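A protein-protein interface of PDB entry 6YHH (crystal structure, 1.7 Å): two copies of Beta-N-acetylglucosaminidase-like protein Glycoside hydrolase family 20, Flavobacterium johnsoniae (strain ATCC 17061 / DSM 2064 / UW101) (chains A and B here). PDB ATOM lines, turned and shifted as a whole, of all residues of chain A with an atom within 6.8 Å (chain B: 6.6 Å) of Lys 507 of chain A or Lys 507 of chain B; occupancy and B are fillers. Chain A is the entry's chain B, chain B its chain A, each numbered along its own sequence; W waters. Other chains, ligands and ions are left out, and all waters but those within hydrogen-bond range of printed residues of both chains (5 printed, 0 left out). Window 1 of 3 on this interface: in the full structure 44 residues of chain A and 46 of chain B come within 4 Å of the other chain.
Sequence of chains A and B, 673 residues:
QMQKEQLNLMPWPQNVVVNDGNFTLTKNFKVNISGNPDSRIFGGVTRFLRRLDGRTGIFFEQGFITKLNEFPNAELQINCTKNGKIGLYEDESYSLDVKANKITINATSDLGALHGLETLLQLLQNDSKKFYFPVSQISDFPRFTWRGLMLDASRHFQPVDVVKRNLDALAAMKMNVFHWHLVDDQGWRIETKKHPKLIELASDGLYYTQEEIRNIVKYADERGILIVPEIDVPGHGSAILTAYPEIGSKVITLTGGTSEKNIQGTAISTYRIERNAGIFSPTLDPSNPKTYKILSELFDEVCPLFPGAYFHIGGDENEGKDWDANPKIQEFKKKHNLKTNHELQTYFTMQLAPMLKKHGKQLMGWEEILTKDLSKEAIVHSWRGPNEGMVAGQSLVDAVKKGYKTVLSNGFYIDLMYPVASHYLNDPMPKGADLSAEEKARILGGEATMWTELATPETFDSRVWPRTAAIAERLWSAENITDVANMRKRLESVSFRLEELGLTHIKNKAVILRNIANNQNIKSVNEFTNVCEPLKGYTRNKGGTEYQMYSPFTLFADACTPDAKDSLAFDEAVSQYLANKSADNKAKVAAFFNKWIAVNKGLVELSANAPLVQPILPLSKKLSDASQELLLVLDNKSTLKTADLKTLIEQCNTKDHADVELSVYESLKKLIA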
ATOM      1  N   GLU A 458     -24.165  -8.641  -9.197  1.00  0.00           N
ATOM      2  CA  GLU A 458     -24.196  -7.196  -9.136  1.00  0.00           C
ATOM      3  C   GLU A 458     -25.335  -6.614  -9.915  1.00  0.00           C
ATOM      4  O   GLU A 458     -25.939  -5.624  -9.483  1.00  0.00           O
ATOM      5  CB  GLU A 458     -22.922  -6.578  -9.579  1.00  0.00           C
ATOM      6  CG  GLU A 458     -21.717  -6.862  -8.689  1.00  0.00           C
ATOM      7  CD  GLU A 458     -21.157  -8.245  -8.823  1.00  0.00           C
ATOM      8  OE1 GLU A 458     -21.292  -8.895  -9.858  1.00  0.00           O
ATOM      9  OE2 GLU A 458     -20.617  -8.739  -7.841  1.00  0.00           O
ATOM     10  N   GLU A 499     -35.411  -0.660  -1.558  1.00  0.00           N
ATOM     11  CA  GLU A 499     -34.033  -0.505  -1.205  1.00  0.00           C
ATOM     12  C   GLU A 499     -33.744  -0.816   0.259  1.00  0.00           C
ATOM     13  O   GLU A 499     -32.632  -1.166   0.638  1.00  0.00           O
ATOM     14  CB  GLU A 499     -33.506   0.922  -1.534  1.00  0.00           C
ATOM     15  CG  GLU A 499     -33.561   1.285  -2.987  1.00  0.00           C
ATOM     16  CD  GLU A 499     -32.677   2.484  -3.205  1.00  0.00           C
ATOM     17  OE1 GLU A 499     -33.114   3.581  -2.827  1.00  0.00           O
ATOM     18  OE2 GLU A 499     -31.584   2.373  -3.784  1.00  0.00           O
ATOM     19  N   GLY A 502     -32.217  -4.157   0.896  1.00  0.00           N
ATOM     20  CA  GLY A 502     -30.911  -4.381   0.336  1.00  0.00           C
ATOM     21  C   GLY A 502     -30.903  -4.544  -1.168  1.00  0.00           C
ATOM     22  O   GLY A 502     -29.806  -4.744  -1.753  1.00  0.00           O
ATOM     23  N   LEU A 503     -32.060  -4.431  -1.811  1.00  0.00           N
ATOM     24  CA  LEU A 503     -32.130  -4.566  -3.261  1.00  0.00           C
ATOM     25  C   LEU A 503     -31.236  -3.493  -3.931  1.00  0.00           C
ATOM     26  O   LEU A 503     -31.218  -2.339  -3.504  1.00  0.00           O
ATOM     27  CB  LEU A 503     -33.567  -4.500  -3.788  1.00  0.00           C
ATOM     28  CG  LEU A 503     -34.487  -5.678  -3.481  1.00  0.00           C
ATOM     29  CD1 LEU A 503     -35.800  -5.401  -4.172  1.00  0.00           C
ATOM     30  CD2 LEU A 503     -33.867  -7.017  -3.884  1.00  0.00           C
ATOM     31  N   THR A 504     -30.469  -3.908  -4.964  1.00  0.00           N
ATOM     32  CA  THR A 504     -29.415  -3.101  -5.554  1.00  0.00           C
ATOM     33  C   THR A 504     -29.776  -2.387  -6.835  1.00  0.00           C
ATOM     34  O   THR A 504     -28.898  -1.835  -7.521  1.00  0.00           O
ATOM     35  CB  THR A 504     -28.127  -3.931  -5.796  1.00  0.00           C
ATOM     36  OG1 THR A 504     -28.306  -4.838  -6.916  1.00  0.00           O
ATOM     37  CG2 THR A 504     -27.716  -4.777  -4.584  1.00  0.00           C
ATOM     38  N   HIS A 505     -31.027  -2.484  -7.225  1.00  0.00           N
ATOM     39  CA  HIS A 505     -31.424  -2.034  -8.573  1.00  0.00           C
ATOM     40  C   HIS A 505     -31.038  -0.596  -8.859  1.00  0.00           C
ATOM     41  O   HIS A 505     -30.602  -0.250  -9.964  1.00  0.00           O
ATOM     42  CB  HIS A 505     -32.891  -2.335  -8.824  1.00  0.00           C
ATOM     43  CG  HIS A 505     -33.800  -1.815  -7.785  1.00  0.00           C
ATOM     44  ND1 HIS A 505     -33.712  -2.202  -6.466  1.00  0.00           N
ATOM     45  CD2 HIS A 505     -34.845  -0.955  -7.851  1.00  0.00           C
ATOM     46  CE1 HIS A 505     -34.663  -1.602  -5.770  1.00  0.00           C
ATOM     47  NE2 HIS A 505     -35.367  -0.857  -6.594  1.00  0.00           N
ATOM     48  N   ILE A 506     -31.171   0.287  -7.899  1.00  0.00           N
ATOM     49  CA  ILE A 506     -30.814   1.689  -8.133  1.00  0.00           C
ATOM     50  C   ILE A 506     -29.357   1.960  -7.787  1.00  0.00           C
ATOM     51  O   ILE A 506     -28.588   2.626  -8.547  1.00  0.00           O
ATOM     52  CB  ILE A 506     -31.712   2.612  -7.237  1.00  0.00           C
ATOM     53  CG1 ILE A 506     -33.148   2.346  -7.538  1.00  0.00           C
ATOM     54  CG2 ILE A 506     -31.389   4.049  -7.563  1.00  0.00           C
ATOM     55  CD1 ILE A 506     -34.201   2.775  -6.584  1.00  0.00           C
ATOM     56  N   LYS A 507     -28.882   1.437  -6.658  1.00  0.00           N
ATOM     57  CA  LYS A 507     -27.586   1.810  -6.167  1.00  0.00           C
ATOM     58  C   LYS A 507     -26.417   1.210  -6.970  1.00  0.00           C
ATOM     59  O   LYS A 507     -25.341   1.864  -7.129  1.00  0.00           O
ATOM     60  CB  LYS A 507     -27.417   1.512  -4.682  1.00  0.00           C
ATOM     61  CG  LYS A 507     -27.247   0.066  -4.304  1.00  0.00           C
ATOM     62  CD  LYS A 507     -27.518  -0.107  -2.810  1.00  0.00           C
ATOM     63  CE  LYS A 507     -27.362  -1.483  -2.279  1.00  0.00           C
ATOM     64  NZ  LYS A 507     -27.514  -1.598  -0.812  1.00  0.00           N
ATOM     65  N   ASN A 508     -26.592   0.016  -7.521  1.00  0.00           N
ATOM     66  CA  ASN A 508     -25.458  -0.608  -8.184  1.00  0.00           C
ATOM     67  C   ASN A 508     -25.218   0.052  -9.521  1.00  0.00           C
ATOM     68  O   ASN A 508     -24.159  -0.120 -10.123  1.00  0.00           O
ATOM     69  CB  ASN A 508     -25.588  -2.123  -8.299  1.00  0.00           C
ATOM     70  CG  ASN A 508     -25.085  -2.852  -7.066  1.00  0.00           C
ATOM     71  OD1 ASN A 508     -24.681  -2.206  -6.061  1.00  0.00           O
ATOM     72  ND2 ASN A 508     -25.129  -4.160  -7.087  1.00  0.00           N
ATOM     73  N   LYS A 509     -26.207   0.767 -10.041  1.00  0.00           N
ATOM     74  CA  LYS A 509     -26.042   1.496 -11.266  1.00  0.00           C
ATOM     75  C   LYS A 509     -24.956   2.555 -11.132  1.00  0.00           C
ATOM     76  O   LYS A 509     -24.150   2.767 -12.058  1.00  0.00           O
ATOM     77  CB  LYS A 509     -27.398   2.137 -11.622  1.00  0.00           C
ATOM     78  CG  LYS A 509     -27.382   3.094 -12.756  1.00  0.00           C
ATOM     79  CD  LYS A 509     -28.742   3.731 -12.948  1.00  0.00           C
ATOM     80  CE  LYS A 509     -28.789   4.476 -14.219  1.00  0.00           C
ATOM     81  NZ  LYS A 509     -30.107   5.017 -14.568  1.00  0.00           N
ATOM     82  N   ALA A 510     -24.955   3.250  -9.976  1.00  0.00           N
ATOM     83  CA  ALA A 510     -23.912   4.254  -9.758  1.00  0.00           C
ATOM     84  C   ALA A 510     -22.510   3.652  -9.740  1.00  0.00           C
ATOM     85  O   ALA A 510     -21.562   4.306 -10.168  1.00  0.00           O
ATOM     86  CB  ALA A 510     -24.242   4.976  -8.452  1.00  0.00           C
ATOM     87  N   VAL A 511     -22.332   2.434  -9.206  1.00  0.00           N
ATOM     88  CA  VAL A 511     -21.065   1.743  -9.193  1.00  0.00           C
ATOM     89  C   VAL A 511     -20.524   1.588 -10.638  1.00  0.00           C
ATOM     90  O   VAL A 511     -19.350   1.916 -10.968  1.00  0.00           O
ATOM     91  CB  VAL A 511     -21.170   0.344  -8.552  1.00  0.00           C
ATOM     92  CG1 VAL A 511     -19.857  -0.380  -8.643  1.00  0.00           C
ATOM     93  CG2 VAL A 511     -21.514   0.522  -7.046  1.00  0.00           C
ATOM     94  N   ILE A 512     -21.430   1.112 -11.503  1.00  0.00           N
ATOM     95  CA  ILE A 512     -21.113   0.857 -12.898  1.00  0.00           C
ATOM     96  C   ILE A 512     -20.748   2.179 -13.547  1.00  0.00           C
ATOM     97  O   ILE A 512     -19.770   2.282 -14.354  1.00  0.00           O
ATOM     98  CB  ILE A 512     -22.284   0.134 -13.606  1.00  0.00           C
ATOM     99  CG1 ILE A 512     -22.391  -1.256 -13.056  1.00  0.00           C
ATOM    100  CG2 ILE A 512     -22.047   0.141 -15.095  1.00  0.00           C
ATOM    101  CD1 ILE A 512     -23.672  -1.961 -13.388  1.00  0.00           C
ATOM    102  N   ARG A 514     -19.608   5.013 -12.213  1.00  0.00           N
ATOM    103  CA  ARG A 514     -18.273   5.383 -11.785  1.00  0.00           C
ATOM    104  C   ARG A 514     -17.180   4.627 -12.515  1.00  0.00           C
ATOM    105  O   ARG A 514     -16.150   5.228 -12.950  1.00  0.00           O
ATOM    106  CB  ARG A 514     -18.092   5.280 -10.211  1.00  0.00           C
ATOM    107  CG  ARG A 514     -18.797   6.461  -9.541  1.00  0.00           C
ATOM    108  CD  ARG A 514     -18.500   6.410  -8.053  1.00  0.00           C
ATOM    109  NE  ARG A 514     -19.344   5.467  -7.343  1.00  0.00           N
ATOM    110  CZ  ARG A 514     -20.603   5.672  -6.937  1.00  0.00           C
ATOM    111  NH1 ARG A 514     -21.240   4.669  -6.312  1.00  0.00           N
ATOM    112  NH2 ARG A 514     -21.249   6.836  -7.133  1.00  0.00           N
ATOM    113  N   GLU B 458     -25.630  -2.148   6.810  1.00  0.00           N
ATOM    114  CA  GLU B 458     -25.764  -1.122   5.752  1.00  0.00           C
ATOM    115  C   GLU B 458     -24.722  -0.048   5.820  1.00  0.00           C
ATOM    116  O   GLU B 458     -24.199   0.448   4.796  1.00  0.00           O
ATOM    117  CB  GLU B 458     -27.192  -0.541   5.711  1.00  0.00           C
ATOM    118  CG  GLU B 458     -28.242  -1.630   5.367  1.00  0.00           C
ATOM    119  CD  GLU B 458     -28.641  -2.566   6.460  1.00  0.00           C
ATOM    120  OE1 GLU B 458     -28.478  -2.270   7.657  1.00  0.00           O
ATOM    121  OE2 GLU B 458     -28.939  -3.734   6.026  1.00  0.00           O
ATOM    122  N   GLU B 499     -15.059  -0.469  -4.850  1.00  0.00           N
ATOM    123  CA  GLU B 499     -16.470  -0.752  -5.135  1.00  0.00           C
ATOM    124  C   GLU B 499     -16.661  -1.994  -5.950  1.00  0.00           C
ATOM    125  O   GLU B 499     -17.710  -2.644  -5.872  1.00  0.00           O
ATOM    126  CB  GLU B 499     -17.148   0.401  -5.849  1.00  0.00           C
ATOM    127  CG  GLU B 499     -17.361   1.667  -5.016  1.00  0.00           C
ATOM    128  CD  GLU B 499     -18.315   2.612  -5.659  1.00  0.00           C
ATOM    129  OE1 GLU B 499     -18.039   3.046  -6.770  1.00  0.00           O
ATOM    130  OE2 GLU B 499     -19.411   2.766  -5.055  1.00  0.00           O
ATOM    131  N   GLY B 502     -17.701  -4.988  -3.988  1.00  0.00           N
ATOM    132  CA  GLY B 502     -18.999  -4.920  -3.312  1.00  0.00           C
ATOM    133  C   GLY B 502     -19.058  -3.959  -2.161  1.00  0.00           C
ATOM    134  O   GLY B 502     -20.107  -3.811  -1.513  1.00  0.00           O
ATOM    135  N   LEU B 503     -17.959  -3.281  -1.859  1.00  0.00           N
ATOM    136  CA  LEU B 503     -17.981  -2.379  -0.695  1.00  0.00           C
ATOM    137  C   LEU B 503     -18.988  -1.264  -0.891  1.00  0.00           C
ATOM    138  O   LEU B 503     -19.159  -0.711  -1.989  1.00  0.00           O
ATOM    139  CB  LEU B 503     -16.542  -1.779  -0.413  1.00  0.00           C
ATOM    140  CG  LEU B 503     -15.575  -2.667   0.402  1.00  0.00           C
ATOM    141  CD1 LEU B 503     -16.032  -3.355   1.633  1.00  0.00           C
ATOM    142  CD2 LEU B 503     -15.255  -3.882  -0.461  1.00  0.00           C
ATOM    143  N   THR B 504     -19.705  -0.902   0.157  1.00  0.00           N
ATOM    144  CA  THR B 504     -20.933  -0.105   0.027  1.00  0.00           C
ATOM    145  C   THR B 504     -20.722   1.300   0.498  1.00  0.00           C
ATOM    146  O   THR B 504     -21.676   2.055   0.635  1.00  0.00           O
ATOM    147  CB  THR B 504     -22.083  -0.649   0.886  1.00  0.00           C
ATOM    148  OG1 THR B 504     -21.810  -0.509   2.299  1.00  0.00           O
ATOM    149  CG2 THR B 504     -22.363  -2.137   0.627  1.00  0.00           C
ATOM    150  N   HIS B 505     -19.480   1.680   0.781  1.00  0.00           N
ATOM    151  CA  HIS B 505     -19.247   2.989   1.420  1.00  0.00           C
ATOM    152  C   HIS B 505     -19.826   4.194   0.653  1.00  0.00           C
ATOM    153  O   HIS B 505     -20.392   5.103   1.244  1.00  0.00           O
ATOM    154  CB  HIS B 505     -17.781   3.213   1.745  1.00  0.00           C
ATOM    155  CG  HIS B 505     -16.856   2.970   0.607  1.00  0.00           C
ATOM    156  ND1 HIS B 505     -16.782   1.753  -0.032  1.00  0.00           N
ATOM    157  CD2 HIS B 505     -15.924   3.764   0.020  1.00  0.00           C
ATOM    158  CE1 HIS B 505     -15.909   1.837  -1.015  1.00  0.00           C
ATOM    159  NE2 HIS B 505     -15.316   3.024  -0.955  1.00  0.00           N
ATOM    160  N   ILE B 506     -19.729   4.179  -0.651  1.00  0.00           N
ATOM    161  CA  ILE B 506     -20.237   5.268  -1.492  1.00  0.00           C
ATOM    162  C   ILE B 506     -21.715   5.001  -1.797  1.00  0.00           C
ATOM    163  O   ILE B 506     -22.583   5.897  -1.657  1.00  0.00           O
ATOM    164  CB  ILE B 506     -19.401   5.410  -2.804  1.00  0.00           C
ATOM    165  CG1 ILE B 506     -17.920   5.677  -2.459  1.00  0.00           C
ATOM    166  CG2 ILE B 506     -19.917   6.576  -3.617  1.00  0.00           C
ATOM    167  CD1 ILE B 506     -16.967   5.409  -3.591  1.00  0.00           C
ATOM    168  N   LYS B 507     -22.052   3.795  -2.249  1.00  0.00           N
ATOM    169  CA  LYS B 507     -23.398   3.562  -2.819  1.00  0.00           C
ATOM    170  C   LYS B 507     -24.521   3.523  -1.781  1.00  0.00           C
ATOM    171  O   LYS B 507     -25.646   3.967  -2.070  1.00  0.00           O
ATOM    172  CB  LYS B 507     -23.398   2.281  -3.705  1.00  0.00           C
ATOM    173  CG  LYS B 507     -23.289   0.960  -2.982  1.00  0.00           C
ATOM    174  CD  LYS B 507     -23.027  -0.173  -3.943  1.00  0.00           C
ATOM    175  CE  LYS B 507     -23.058  -1.496  -3.270  1.00  0.00           C
ATOM    176  NZ  LYS B 507     -22.603  -2.622  -4.180  1.00  0.00           N
ATOM    177  N   ASN B 508     -24.243   3.005  -0.574  1.00  0.00           N
ATOM    178  CA  ASN B 508     -25.281   2.935   0.423  1.00  0.00           C
ATOM    179  C   ASN B 508     -25.624   4.342   0.952  1.00  0.00           C
ATOM    180  O   ASN B 508     -26.698   4.546   1.494  1.00  0.00           O
ATOM    181  CB  ASN B 508     -24.922   1.950   1.565  1.00  0.00           C
ATOM    182  CG  ASN B 508     -25.296   0.513   1.267  1.00  0.00           C
ATOM    183  OD1 ASN B 508     -25.198  -0.421   2.187  1.00  0.00           O
ATOM    184  ND2 ASN B 508     -25.701   0.267   0.051  1.00  0.00           N
ATOM    185  N   LYS B 509     -24.746   5.348   0.788  1.00  0.00           N
ATOM    186  CA  LYS B 509     -25.051   6.680   1.192  1.00  0.00           C
ATOM    187  C   LYS B 509     -26.236   7.205   0.407  1.00  0.00           C
ATOM    188  O   LYS B 509     -27.112   7.849   0.946  1.00  0.00           O
ATOM    189  CB  LYS B 509     -23.821   7.577   0.899  1.00  0.00           C
ATOM    190  CG  LYS B 509     -24.002   9.042   1.188  1.00  0.00           C
ATOM    191  CD  LYS B 509     -22.744   9.779   0.786  1.00  0.00           C
ATOM    192  CE  LYS B 509     -22.870  11.225   1.121  1.00  0.00           C
ATOM    193  NZ  LYS B 509     -21.550  11.920   0.979  1.00  0.00           N
ATOM    194  N   ALA B 510     -26.312   6.855  -0.884  1.00  0.00           N
ATOM    195  CA  ALA B 510     -27.453   7.366  -1.707  1.00  0.00           C
ATOM    196  C   ALA B 510     -28.776   6.730  -1.309  1.00  0.00           C
ATOM    197  O   ALA B 510     -29.809   7.356  -1.421  1.00  0.00           O
ATOM    198  CB  ALA B 510     -27.222   7.134  -3.215  1.00  0.00           C
ATOM    199  N   VAL B 511     -28.783   5.479  -0.871  1.00  0.00           N
ATOM    200  CA  VAL B 511     -29.911   4.850  -0.359  1.00  0.00           C
ATOM    201  C   VAL B 511     -30.466   5.612   0.854  1.00  0.00           C
ATOM    202  O   VAL B 511     -31.690   5.869   0.973  1.00  0.00           O
ATOM    203  CB  VAL B 511     -29.617   3.418   0.102  1.00  0.00           C
ATOM    204  CG1 VAL B 511     -30.834   2.809   0.760  1.00  0.00           C
ATOM    205  CG2 VAL B 511     -29.136   2.588  -1.095  1.00  0.00           C
ATOM    206  N   ILE B 512     -29.562   5.950   1.771  1.00  0.00           N
ATOM    207  CA  ILE B 512     -29.937   6.723   2.967  1.00  0.00           C
ATOM    208  C   ILE B 512     -30.478   8.093   2.566  1.00  0.00           C
ATOM    209  O   ILE B 512     -31.503   8.525   3.079  1.00  0.00           O
ATOM    210  CB  ILE B 512     -28.778   6.848   3.944  1.00  0.00           C
ATOM    211  CG1 ILE B 512     -28.514   5.437   4.546  1.00  0.00           C
ATOM    212  CG2 ILE B 512     -29.101   7.789   5.078  1.00  0.00           C
ATOM    213  CD1 ILE B 512     -27.134   5.332   5.170  1.00  0.00           C
ATOM    214  N   ARG B 514     -31.933   8.952  -0.246  1.00  0.00           N
ATOM    215  CA  ARG B 514     -33.314   8.761  -0.809  1.00  0.00           C
ATOM    216  C   ARG B 514     -34.335   8.552   0.283  1.00  0.00           C
ATOM    217  O   ARG B 514     -35.442   9.155   0.241  1.00  0.00           O
ATOM    218  CB  ARG B 514     -33.348   7.652  -1.846  1.00  0.00           C
ATOM    219  CG  ARG B 514     -32.810   8.106  -3.215  1.00  0.00           C
ATOM    220  CD  ARG B 514     -32.978   6.968  -4.242  1.00  0.00           C
ATOM    221  NE  ARG B 514     -32.036   5.844  -4.071  1.00  0.00           N
ATOM    222  CZ  ARG B 514     -30.782   5.784  -4.513  1.00  0.00           C
ATOM    223  NH1 ARG B 514     -30.216   6.814  -5.103  1.00  0.00           N
ATOM    224  NH2 ARG B 514     -30.056   4.708  -4.272  1.00  0.00           N
HETATM  225  O   HOH W   1     -30.402  -3.821   3.744  1.00  0.00           O
HETATM  226  O   HOH W   2     -17.195   2.044  -9.240  1.00  0.00           O
HETATM  227  O   HOH W   3     -19.514  -7.101  -5.994  1.00  0.00           O
HETATM  228  O   HOH W   4     -33.860   4.539  -0.219  1.00  0.00           O
HETATM  229  O   HOH W   5     -21.671  -3.466  -7.200  1.00  0.00           O
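Of the 14 printed residues of chain A, 6 touch a printed residue of chain B. Printed residues of chain A that touch a printed residue of chain B: Glu 499, Ile 506, Lys 507, Asn 508, Val 511 and Arg 514. Hydrophobic or aromatic side chains of chain A that line the printed part of chain B: Ile 506 and Val 511. Of the 14 printed residues of chain B, 6 touch a printed residue of chain A. Hydrophobic or aromatic side chains of chain B that line the printed part of chain A: Ile 506 and Val 511. Among the printed residues, 11 pairs touch across the chains. Among the printed residues, Asp or Glu carboxylates within 4 Å of a Lys or Arg side-chain nitrogen of the other chain: Glu 499 of chain A with Arg 514 of chain B (2.8 Å) and Arg 514 of chain A with Glu 499 of chain B (2.8 Å).
The guanidinium group of Arg 514 of chain A lies within salt-bridge range of the side-chain carboxylate of Glu 499 of chain B (2.8 Å). The side-chain amino group of Lys 507 of chain B lies within hydrogen-bond range of the side-chain amide oxygen of Asn 508 of chain A (2.8 Å). The side-chain amino group (NZ) of Lys 507 of chain A lies close to the side-chain amide nitrogen (ND2) of Asn 508 of chain B. NE of Arg 514 of chain B lies within salt-bridge range of OE1 of Glu 499 of chain A.
Among the printed residues, pairs that only touch across the chains: Arg 514 of chain A with Ile 506 of chain B, Val 511 of chain A with Lys 507 of chain B, Ile 506 of chain A with Arg 514 of chain B, Lys 507 of chain A with Val 511 of chain B, Glu 499 of chain A with Val 511 of chain B, Val 511 of chain A with Glu 499 of chain B and Lys 507 of chain A with Lys 507 of chain B.
Glu 499 of chain A touches Val 511 of chain B, and with the chains exchanged Val 511 of chain A touches Glu 499 of chain B. Glu 499 of chain A touches Arg 514 of chain B, and with the chains exchanged Arg 514 of chain A touches Glu 499 of chain B. Ile 506 of chain A touches Arg 514 of chain B, and with the chains exchanged Arg 514 of chain A touches Ile 506 of chain B. Lys 507 of chain B touches its own counterpart, Lys 507 of chain A.
Lys 507 of chain A touches just these residues of chain B: Lys 507 (3.96 Å), Asn 508 (2.7 Å) and Val 511 (3.6 Å). Lys 507 of chain B touches three residues of chain A. Of the printed residues of chain B, Arg 514 of chain A touches Glu 499 (2.8 Å) and Ile 506 (3.5 Å). Of the printed residues of chain A, Asn 508 of chain B touches Lys 507. Of the printed residues of chain A, Ile 506 of chain B touches Arg 514. His 505 of chain B touches none of the printed residues of chain A.
Water W3 bridges OE2 of Glu 458 of chain A (2.7 Å) and N of Gly 502 of chain B (3.4 Å). Water W1 bridges OE2 of Glu 458 of chain B and N of Gly 502 of chain A. Water W2 bridges O of Val 511 of chain A (2.8 Å) and OE1 of Glu 499 of chain B (2.8 Å). Water W4 bridges O of Val 511 of chain B and OE1 of Glu 499 of chain A. Water W5 bridges NZ of Lys 507 of chain B (3.3 Å) and OD1 of Asn 508 of chain A (3.5 Å).
The side-chain amide oxygen (OD1) of Asn 508 of chain B lies close to the backbone carbonyl oxygen (O) of Glu 458 of chain B (2.9 Å). OG1 of Thr 504 of chain B sits close to OD1 of Asn 508 of chain B. O of Glu 458 of chain A lies within hydrogen-bond range of ND2 of Asn 508 of chain A (2.9 Å). ND2 of Asn 508 of chain A sits at hydrogen-bond distance from OG1 of Thr 504 of chain A, 3.3 Å away.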
